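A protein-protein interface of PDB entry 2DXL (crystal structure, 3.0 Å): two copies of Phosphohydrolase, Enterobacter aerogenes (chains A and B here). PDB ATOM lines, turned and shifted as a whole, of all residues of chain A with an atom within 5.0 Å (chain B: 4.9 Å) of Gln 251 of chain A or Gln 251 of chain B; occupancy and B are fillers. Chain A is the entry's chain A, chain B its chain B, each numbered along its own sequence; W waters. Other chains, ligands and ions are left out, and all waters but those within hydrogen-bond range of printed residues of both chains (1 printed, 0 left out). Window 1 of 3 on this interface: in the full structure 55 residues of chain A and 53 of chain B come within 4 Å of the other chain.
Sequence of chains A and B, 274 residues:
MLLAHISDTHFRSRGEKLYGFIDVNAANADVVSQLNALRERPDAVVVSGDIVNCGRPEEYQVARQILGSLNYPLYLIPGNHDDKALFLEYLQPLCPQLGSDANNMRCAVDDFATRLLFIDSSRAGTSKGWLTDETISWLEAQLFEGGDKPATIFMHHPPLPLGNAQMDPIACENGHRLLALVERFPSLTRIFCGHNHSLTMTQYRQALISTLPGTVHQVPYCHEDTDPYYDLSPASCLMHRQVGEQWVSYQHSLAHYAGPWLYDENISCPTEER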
ATOM      1  N   SER A 198     -27.213  24.797   6.959  1.00  0.00           N
ATOM      2  CA  SER A 198     -26.160  25.280   6.112  1.00  0.00           C
ATOM      3  C   SER A 198     -26.182  24.463   4.858  1.00  0.00           C
ATOM      4  O   SER A 198     -26.517  23.279   4.895  1.00  0.00           O
ATOM      5  CB  SER A 198     -24.823  25.032   6.796  1.00  0.00           C
ATOM      6  OG  SER A 198     -23.777  25.321   5.899  1.00  0.00           O
ATOM      7  N   LEU A 199     -25.811  25.073   3.740  1.00  0.00           N
ATOM      8  CA  LEU A 199     -25.521  24.280   2.563  1.00  0.00           C
ATOM      9  C   LEU A 199     -24.048  23.888   2.538  1.00  0.00           C
ATOM     10  O   LEU A 199     -23.176  24.659   2.107  1.00  0.00           O
ATOM     11  CB  LEU A 199     -25.925  24.994   1.278  1.00  0.00           C
ATOM     12  CG  LEU A 199     -26.244  23.965   0.192  1.00  0.00           C
ATOM     13  CD1 LEU A 199     -27.438  24.399  -0.626  1.00  0.00           C
ATOM     14  CD2 LEU A 199     -25.043  23.636  -0.690  1.00  0.00           C
ATOM     15  N   PRO A 213     -29.566  24.555   4.287  1.00  0.00           N
ATOM     16  CA  PRO A 213     -29.922  25.674   5.168  1.00  0.00           C
ATOM     17  C   PRO A 213     -31.274  25.435   5.874  1.00  0.00           C
ATOM     18  O   PRO A 213     -32.097  24.638   5.400  1.00  0.00           O
ATOM     19  CB  PRO A 213     -30.001  26.870   4.211  1.00  0.00           C
ATOM     20  CG  PRO A 213     -29.958  26.310   2.835  1.00  0.00           C
ATOM     21  CD  PRO A 213     -29.283  24.997   2.909  1.00  0.00           C
ATOM     22  N   SER A 236     -33.052  29.666   2.686  1.00  0.00           N
ATOM     23  CA  SER A 236     -33.363  29.196   1.359  1.00  0.00           C
ATOM     24  C   SER A 236     -33.772  27.770   1.484  1.00  0.00           C
ATOM     25  O   SER A 236     -33.727  27.190   2.571  1.00  0.00           O
ATOM     26  CB  SER A 236     -32.132  29.275   0.470  1.00  0.00           C
ATOM     27  OG  SER A 236     -30.976  28.889   1.189  1.00  0.00           O
ATOM     28  N   CYS A 237     -34.165  27.186   0.365  1.00  0.00           N
ATOM     29  CA  CYS A 237     -34.343  25.747   0.333  1.00  0.00           C
ATOM     30  C   CYS A 237     -33.746  25.182  -0.936  1.00  0.00           C
ATOM     31  O   CYS A 237     -33.201  25.920  -1.776  1.00  0.00           O
ATOM     32  CB  CYS A 237     -35.818  25.396   0.400  1.00  0.00           C
ATOM     33  SG  CYS A 237     -36.630  25.889  -1.085  1.00  0.00           S
ATOM     34  N   LEU A 238     -33.880  23.870  -1.070  1.00  0.00           N
ATOM     35  CA  LEU A 238     -33.399  23.170  -2.228  1.00  0.00           C
ATOM     36  C   LEU A 238     -34.585  22.698  -3.059  1.00  0.00           C
ATOM     37  O   LEU A 238     -35.547  22.146  -2.524  1.00  0.00           O
ATOM     38  CB  LEU A 238     -32.527  22.004  -1.775  1.00  0.00           C
ATOM     39  CG  LEU A 238     -31.086  21.991  -2.293  1.00  0.00           C
ATOM     40  CD1 LEU A 238     -30.571  23.389  -2.581  1.00  0.00           C
ATOM     41  CD2 LEU A 238     -30.175  21.282  -1.321  1.00  0.00           C
ATOM     42  N   SER A 249     -30.165  19.752  -8.177  1.00  0.00           N
ATOM     43  CA  SER A 249     -30.643  20.502  -7.037  1.00  0.00           C
ATOM     44  C   SER A 249     -30.160  21.923  -7.209  1.00  0.00           C
ATOM     45  O   SER A 249     -28.996  22.148  -7.546  1.00  0.00           O
ATOM     46  CB  SER A 249     -30.099  19.899  -5.762  1.00  0.00           C
ATOM     47  OG  SER A 249     -30.166  18.494  -5.874  1.00  0.00           O
ATOM     48  N   TYR A 250     -31.076  22.871  -7.026  1.00  0.00           N
ATOM     49  CA  TYR A 250     -30.749  24.288  -7.079  1.00  0.00           C
ATOM     50  C   TYR A 250     -31.370  25.012  -5.919  1.00  0.00           C
ATOM     51  O   TYR A 250     -32.505  24.730  -5.521  1.00  0.00           O
ATOM     52  CB  TYR A 250     -31.203  24.928  -8.384  1.00  0.00           C
ATOM     53  CG  TYR A 250     -32.669  24.787  -8.718  1.00  0.00           C
ATOM     54  CD1 TYR A 250     -33.568  25.834  -8.482  1.00  0.00           C
ATOM     55  CD2 TYR A 250     -33.154  23.620  -9.307  1.00  0.00           C
ATOM     56  CE1 TYR A 250     -34.924  25.719  -8.816  1.00  0.00           C
ATOM     57  CE2 TYR A 250     -34.496  23.484  -9.639  1.00  0.00           C
ATOM     58  CZ  TYR A 250     -35.377  24.536  -9.395  1.00  0.00           C
ATOM     59  OH  TYR A 250     -36.700  24.379  -9.744  1.00  0.00           O
ATOM     60  N   GLN A 251     -30.600  25.946  -5.385  1.00  0.00           N
ATOM     61  CA  GLN A 251     -31.003  26.760  -4.257  1.00  0.00           C
ATOM     62  C   GLN A 251     -32.073  27.782  -4.639  1.00  0.00           C
ATOM     63  O   GLN A 251     -31.917  28.568  -5.592  1.00  0.00           O
ATOM     64  CB  GLN A 251     -29.786  27.469  -3.713  1.00  0.00           C
ATOM     65  CG  GLN A 251     -30.063  28.300  -2.518  1.00  0.00           C
ATOM     66  CD  GLN A 251     -28.801  28.548  -1.746  1.00  0.00           C
ATOM     67  OE1 GLN A 251     -27.914  29.268  -2.208  1.00  0.00           O
ATOM     68  NE2 GLN A 251     -28.694  27.936  -0.567  1.00  0.00           N
ATOM     69  N   HIS A 252     -33.167  27.753  -3.884  1.00  0.00           N
ATOM     70  CA  HIS A 252     -34.257  28.701  -4.055  1.00  0.00           C
ATOM     71  C   HIS A 252     -34.319  29.617  -2.831  1.00  0.00           C
ATOM     72  O   HIS A 252     -34.670  29.153  -1.724  1.00  0.00           O
ATOM     73  CB  HIS A 252     -35.555  27.940  -4.174  1.00  0.00           C
ATOM     74  CG  HIS A 252     -36.713  28.795  -4.557  1.00  0.00           C
ATOM     75  ND1 HIS A 252     -37.416  29.549  -3.638  1.00  0.00           N
ATOM     76  CD2 HIS A 252     -37.298  29.014  -5.760  1.00  0.00           C
ATOM     77  CE1 HIS A 252     -38.387  30.196  -4.258  1.00  0.00           C
ATOM     78  NE2 HIS A 252     -38.340  29.882  -5.544  1.00  0.00           N
ATOM     79  N   SER A 253     -33.963  30.897  -3.018  1.00  0.00           N
ATOM     80  CA  SER A 253     -33.942  31.848  -1.909  1.00  0.00           C
ATOM     81  C   SER A 253     -35.326  32.033  -1.333  1.00  0.00           C
ATOM     82  O   SER A 253     -36.287  32.113  -2.076  1.00  0.00           O
ATOM     83  CB  SER A 253     -33.421  33.206  -2.361  1.00  0.00           C
ATOM     84  OG  SER A 253     -33.673  34.200  -1.368  1.00  0.00           O
ATOM     85  N   SER B 198     -26.012  31.074  -9.722  1.00  0.00           N
ATOM     86  CA  SER B 198     -26.860  30.245  -8.898  1.00  0.00           C
ATOM     87  C   SER B 198     -26.064  29.093  -8.303  1.00  0.00           C
ATOM     88  O   SER B 198     -25.055  28.653  -8.868  1.00  0.00           O
ATOM     89  CB  SER B 198     -28.003  29.689  -9.737  1.00  0.00           C
ATOM     90  OG  SER B 198     -28.761  28.767  -8.989  1.00  0.00           O
ATOM     91  N   LEU B 199     -26.522  28.606  -7.156  1.00  0.00           N
ATOM     92  CA  LEU B 199     -26.036  27.338  -6.644  1.00  0.00           C
ATOM     93  C   LEU B 199     -26.936  26.244  -7.169  1.00  0.00           C
ATOM     94  O   LEU B 199     -27.971  25.922  -6.584  1.00  0.00           O
ATOM     95  CB  LEU B 199     -26.006  27.321  -5.127  1.00  0.00           C
ATOM     96  CG  LEU B 199     -25.301  26.105  -4.550  1.00  0.00           C
ATOM     97  CD1 LEU B 199     -23.800  26.214  -4.704  1.00  0.00           C
ATOM     98  CD2 LEU B 199     -25.657  26.070  -3.110  1.00  0.00           C
ATOM     99  N   PRO B 213     -23.407  30.781  -7.066  1.00  0.00           N
ATOM    100  CA  PRO B 213     -24.026  32.105  -7.116  1.00  0.00           C
ATOM    101  C   PRO B 213     -22.998  33.204  -7.437  1.00  0.00           C
ATOM    102  O   PRO B 213     -21.791  33.003  -7.257  1.00  0.00           O
ATOM    103  CB  PRO B 213     -24.607  32.275  -5.711  1.00  0.00           C
ATOM    104  CG  PRO B 213     -23.950  31.263  -4.889  1.00  0.00           C
ATOM    105  CD  PRO B 213     -23.608  30.129  -5.765  1.00  0.00           C
ATOM    106  N   SER B 236     -23.550  34.906  -2.159  1.00  0.00           N
ATOM    107  CA  SER B 236     -22.714  34.102  -1.274  1.00  0.00           C
ATOM    108  C   SER B 236     -21.531  33.650  -2.075  1.00  0.00           C
ATOM    109  O   SER B 236     -21.413  34.000  -3.250  1.00  0.00           O
ATOM    110  CB  SER B 236     -23.483  32.881  -0.744  1.00  0.00           C
ATOM    111  OG  SER B 236     -24.361  32.344  -1.725  1.00  0.00           O
ATOM    112  N   CYS B 237     -20.657  32.873  -1.455  1.00  0.00           N
ATOM    113  CA  CYS B 237     -19.651  32.164  -2.222  1.00  0.00           C
ATOM    114  C   CYS B 237     -19.493  30.769  -1.645  1.00  0.00           C
ATOM    115  O   CYS B 237     -20.165  30.421  -0.663  1.00  0.00           O
ATOM    116  CB  CYS B 237     -18.335  32.908  -2.188  1.00  0.00           C
ATOM    117  SG  CYS B 237     -17.710  33.052  -0.535  1.00  0.00           S
ATOM    118  N   LEU B 238     -18.621  29.978  -2.258  1.00  0.00           N
ATOM    119  CA  LEU B 238     -18.301  28.660  -1.757  1.00  0.00           C
ATOM    120  C   LEU B 238     -16.928  28.657  -1.113  1.00  0.00           C
ATOM    121  O   LEU B 238     -15.970  29.170  -1.692  1.00  0.00           O
ATOM    122  CB  LEU B 238     -18.321  27.665  -2.909  1.00  0.00           C
ATOM    123  CG  LEU B 238     -19.359  26.553  -2.886  1.00  0.00           C
ATOM    124  CD1 LEU B 238     -20.655  26.968  -2.224  1.00  0.00           C
ATOM    125  CD2 LEU B 238     -19.584  26.109  -4.286  1.00  0.00           C
ATOM    126  N   SER B 249     -17.416  21.559   0.497  1.00  0.00           N
ATOM    127  CA  SER B 249     -17.739  22.893   0.082  1.00  0.00           C
ATOM    128  C   SER B 249     -18.914  23.382   0.902  1.00  0.00           C
ATOM    129  O   SER B 249     -19.922  22.682   1.018  1.00  0.00           O
ATOM    130  CB  SER B 249     -18.137  22.884  -1.384  1.00  0.00           C
ATOM    131  OG  SER B 249     -17.077  22.406  -2.169  1.00  0.00           O
ATOM    132  N   TYR B 250     -18.797  24.584   1.459  1.00  0.00           N
ATOM    133  CA  TYR B 250     -19.919  25.185   2.172  1.00  0.00           C
ATOM    134  C   TYR B 250     -20.176  26.607   1.744  1.00  0.00           C
ATOM    135  O   TYR B 250     -19.263  27.331   1.346  1.00  0.00           O
ATOM    136  CB  TYR B 250     -19.726  25.119   3.677  1.00  0.00           C
ATOM    137  CG  TYR B 250     -18.436  25.699   4.205  1.00  0.00           C
ATOM    138  CD1 TYR B 250     -18.405  26.979   4.772  1.00  0.00           C
ATOM    139  CD2 TYR B 250     -17.251  24.955   4.181  1.00  0.00           C
ATOM    140  CE1 TYR B 250     -17.221  27.517   5.301  1.00  0.00           C
ATOM    141  CE2 TYR B 250     -16.062  25.483   4.694  1.00  0.00           C
ATOM    142  CZ  TYR B 250     -16.058  26.766   5.251  1.00  0.00           C
ATOM    143  OH  TYR B 250     -14.888  27.281   5.756  1.00  0.00           O
ATOM    144  N   GLN B 251     -21.443  26.986   1.790  1.00  0.00           N
ATOM    145  CA  GLN B 251     -21.860  28.300   1.366  1.00  0.00           C
ATOM    146  C   GLN B 251     -21.552  29.304   2.460  1.00  0.00           C
ATOM    147  O   GLN B 251     -21.797  29.072   3.645  1.00  0.00           O
ATOM    148  CB  GLN B 251     -23.343  28.269   1.053  1.00  0.00           C
ATOM    149  CG  GLN B 251     -23.957  29.607   0.747  1.00  0.00           C
ATOM    150  CD  GLN B 251     -25.139  29.460  -0.172  1.00  0.00           C
ATOM    151  OE1 GLN B 251     -26.233  29.101   0.259  1.00  0.00           O
ATOM    152  NE2 GLN B 251     -24.916  29.700  -1.462  1.00  0.00           N
ATOM    153  N   HIS B 252     -20.989  30.427   2.065  1.00  0.00           N
ATOM    154  CA  HIS B 252     -20.653  31.463   3.022  1.00  0.00           C
ATOM    155  C   HIS B 252     -21.351  32.721   2.546  1.00  0.00           C
ATOM    156  O   HIS B 252     -21.011  33.251   1.471  1.00  0.00           O
ATOM    157  CB  HIS B 252     -19.146  31.653   3.055  1.00  0.00           C
ATOM    158  CG  HIS B 252     -18.689  32.699   4.010  1.00  0.00           C
ATOM    159  ND1 HIS B 252     -18.750  34.045   3.721  1.00  0.00           N
ATOM    160  CD2 HIS B 252     -18.150  32.603   5.245  1.00  0.00           C
ATOM    161  CE1 HIS B 252     -18.276  34.739   4.739  1.00  0.00           C
ATOM    162  NE2 HIS B 252     -17.900  33.886   5.675  1.00  0.00           N
ATOM    163  N   SER B 253     -22.348  33.165   3.322  1.00  0.00           N
ATOM    164  CA  SER B 253     -23.169  34.315   2.951  1.00  0.00           C
ATOM    165  C   SER B 253     -22.326  35.570   2.802  1.00  0.00           C
ATOM    166  O   SER B 253     -21.477  35.838   3.639  1.00  0.00           O
ATOM    167  CB  SER B 253     -24.237  34.569   4.005  1.00  0.00           C
ATOM    168  OG  SER B 253     -24.883  35.798   3.746  1.00  0.00           O
HETATM  169  O   HOH W   1     -27.894  30.026  -5.288  1.00  0.00           O
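The backbone NH (N) of Gln 251 of chain B lies within hydrogen-bond range of the backbone carbonyl oxygen (O) of Leu 199 of chain A (2.9 Å). N of Gln 251 of chain A lies within hydrogen-bond range of O of Leu 199 of chain B (2.9 Å). The side-chain amide nitrogen (NE2) of Gln 251 of chain A sits at hydrogen-bond distance from the side-chain amide oxygen (OE1) of Gln 251 of chain B, at 2.8 Å.
The side-chain hydroxyl (OG) of Ser 236 of chain A is in hydrogen-bond range of the side-chain amide nitrogen (NE2) of Gln 251 of chain A (3.0 Å). OG of Ser 236 of chain B sits at hydrogen-bond distance from NE2 of Gln 251 of chain B (2.7 Å).
Among the printed residues, pairs that only touch across the chains: Leu 199 of chain A with Leu 199 of chain B (3.5 Å), Leu 199 of chain A with Ser 249 of chain B (3.96 Å), Leu 199 of chain A with Tyr 250 of chain B (3.3 Å) and Tyr 250 of chain A with Leu 199 of chain B (3.3 Å).
Gln 251 of chain A touches just these residues of chain B: Leu 199 and Gln 251. Gln 251 of chain B touches just these residues of chain A: Leu 199 and Gln 251. Of the printed residues of chain B, Leu 199 of chain A touches Leu 199 (3.5 Å), Ser 249 (3.96 Å), Tyr 250 (3.3 Å) and Gln 251 (2.9 Å). Of the printed residues of chain A, Tyr 250 of chain B touches Leu 199 (3.3 Å). Of the printed residues of chain A, Leu 199 of chain B touches Leu 199 (3.5 Å), Tyr 250 (3.3 Å) and Gln 251 (2.9 Å). Ser 198 of chain B touches none of the printed residues of chain A.
Hydrophobic or aromatic side chains of chain A that line the printed part of chain B: Leu 199 and Tyr 250. Of the 11 printed residues of chain B, 4 touch a printed residue of chain A. Printed residues of chain B that touch a printed residue of chain A: Leu 199, Ser 249, Tyr 250 and Gln 251. Along chain B the printed residues that touch a printed residue of chain A span positions 199 to 251. Among the printed residues, 7 pairs touch across the chains.
Leu 199 of chain A touches its own counterpart, Leu 199 of chain B. Leu 199 of chain A touches Tyr 250 of chain B, and with the chains exchanged Tyr 250 of chain A touches Leu 199 of chain B. Leu 199 of chain A touches Gln 251 of chain B, and with the chains exchanged Gln 251 of chain A touches Leu 199 of chain B. Gln 251 of chain B touches its own counterpart, Gln 251 of chain A. 11 positions are printed for both chains.
Water W1 lies within hydrogen-bond range of N of Leu 199 of chain B (2.7 Å) and OE1 of Gln 251 of chain A (3.2 Å).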
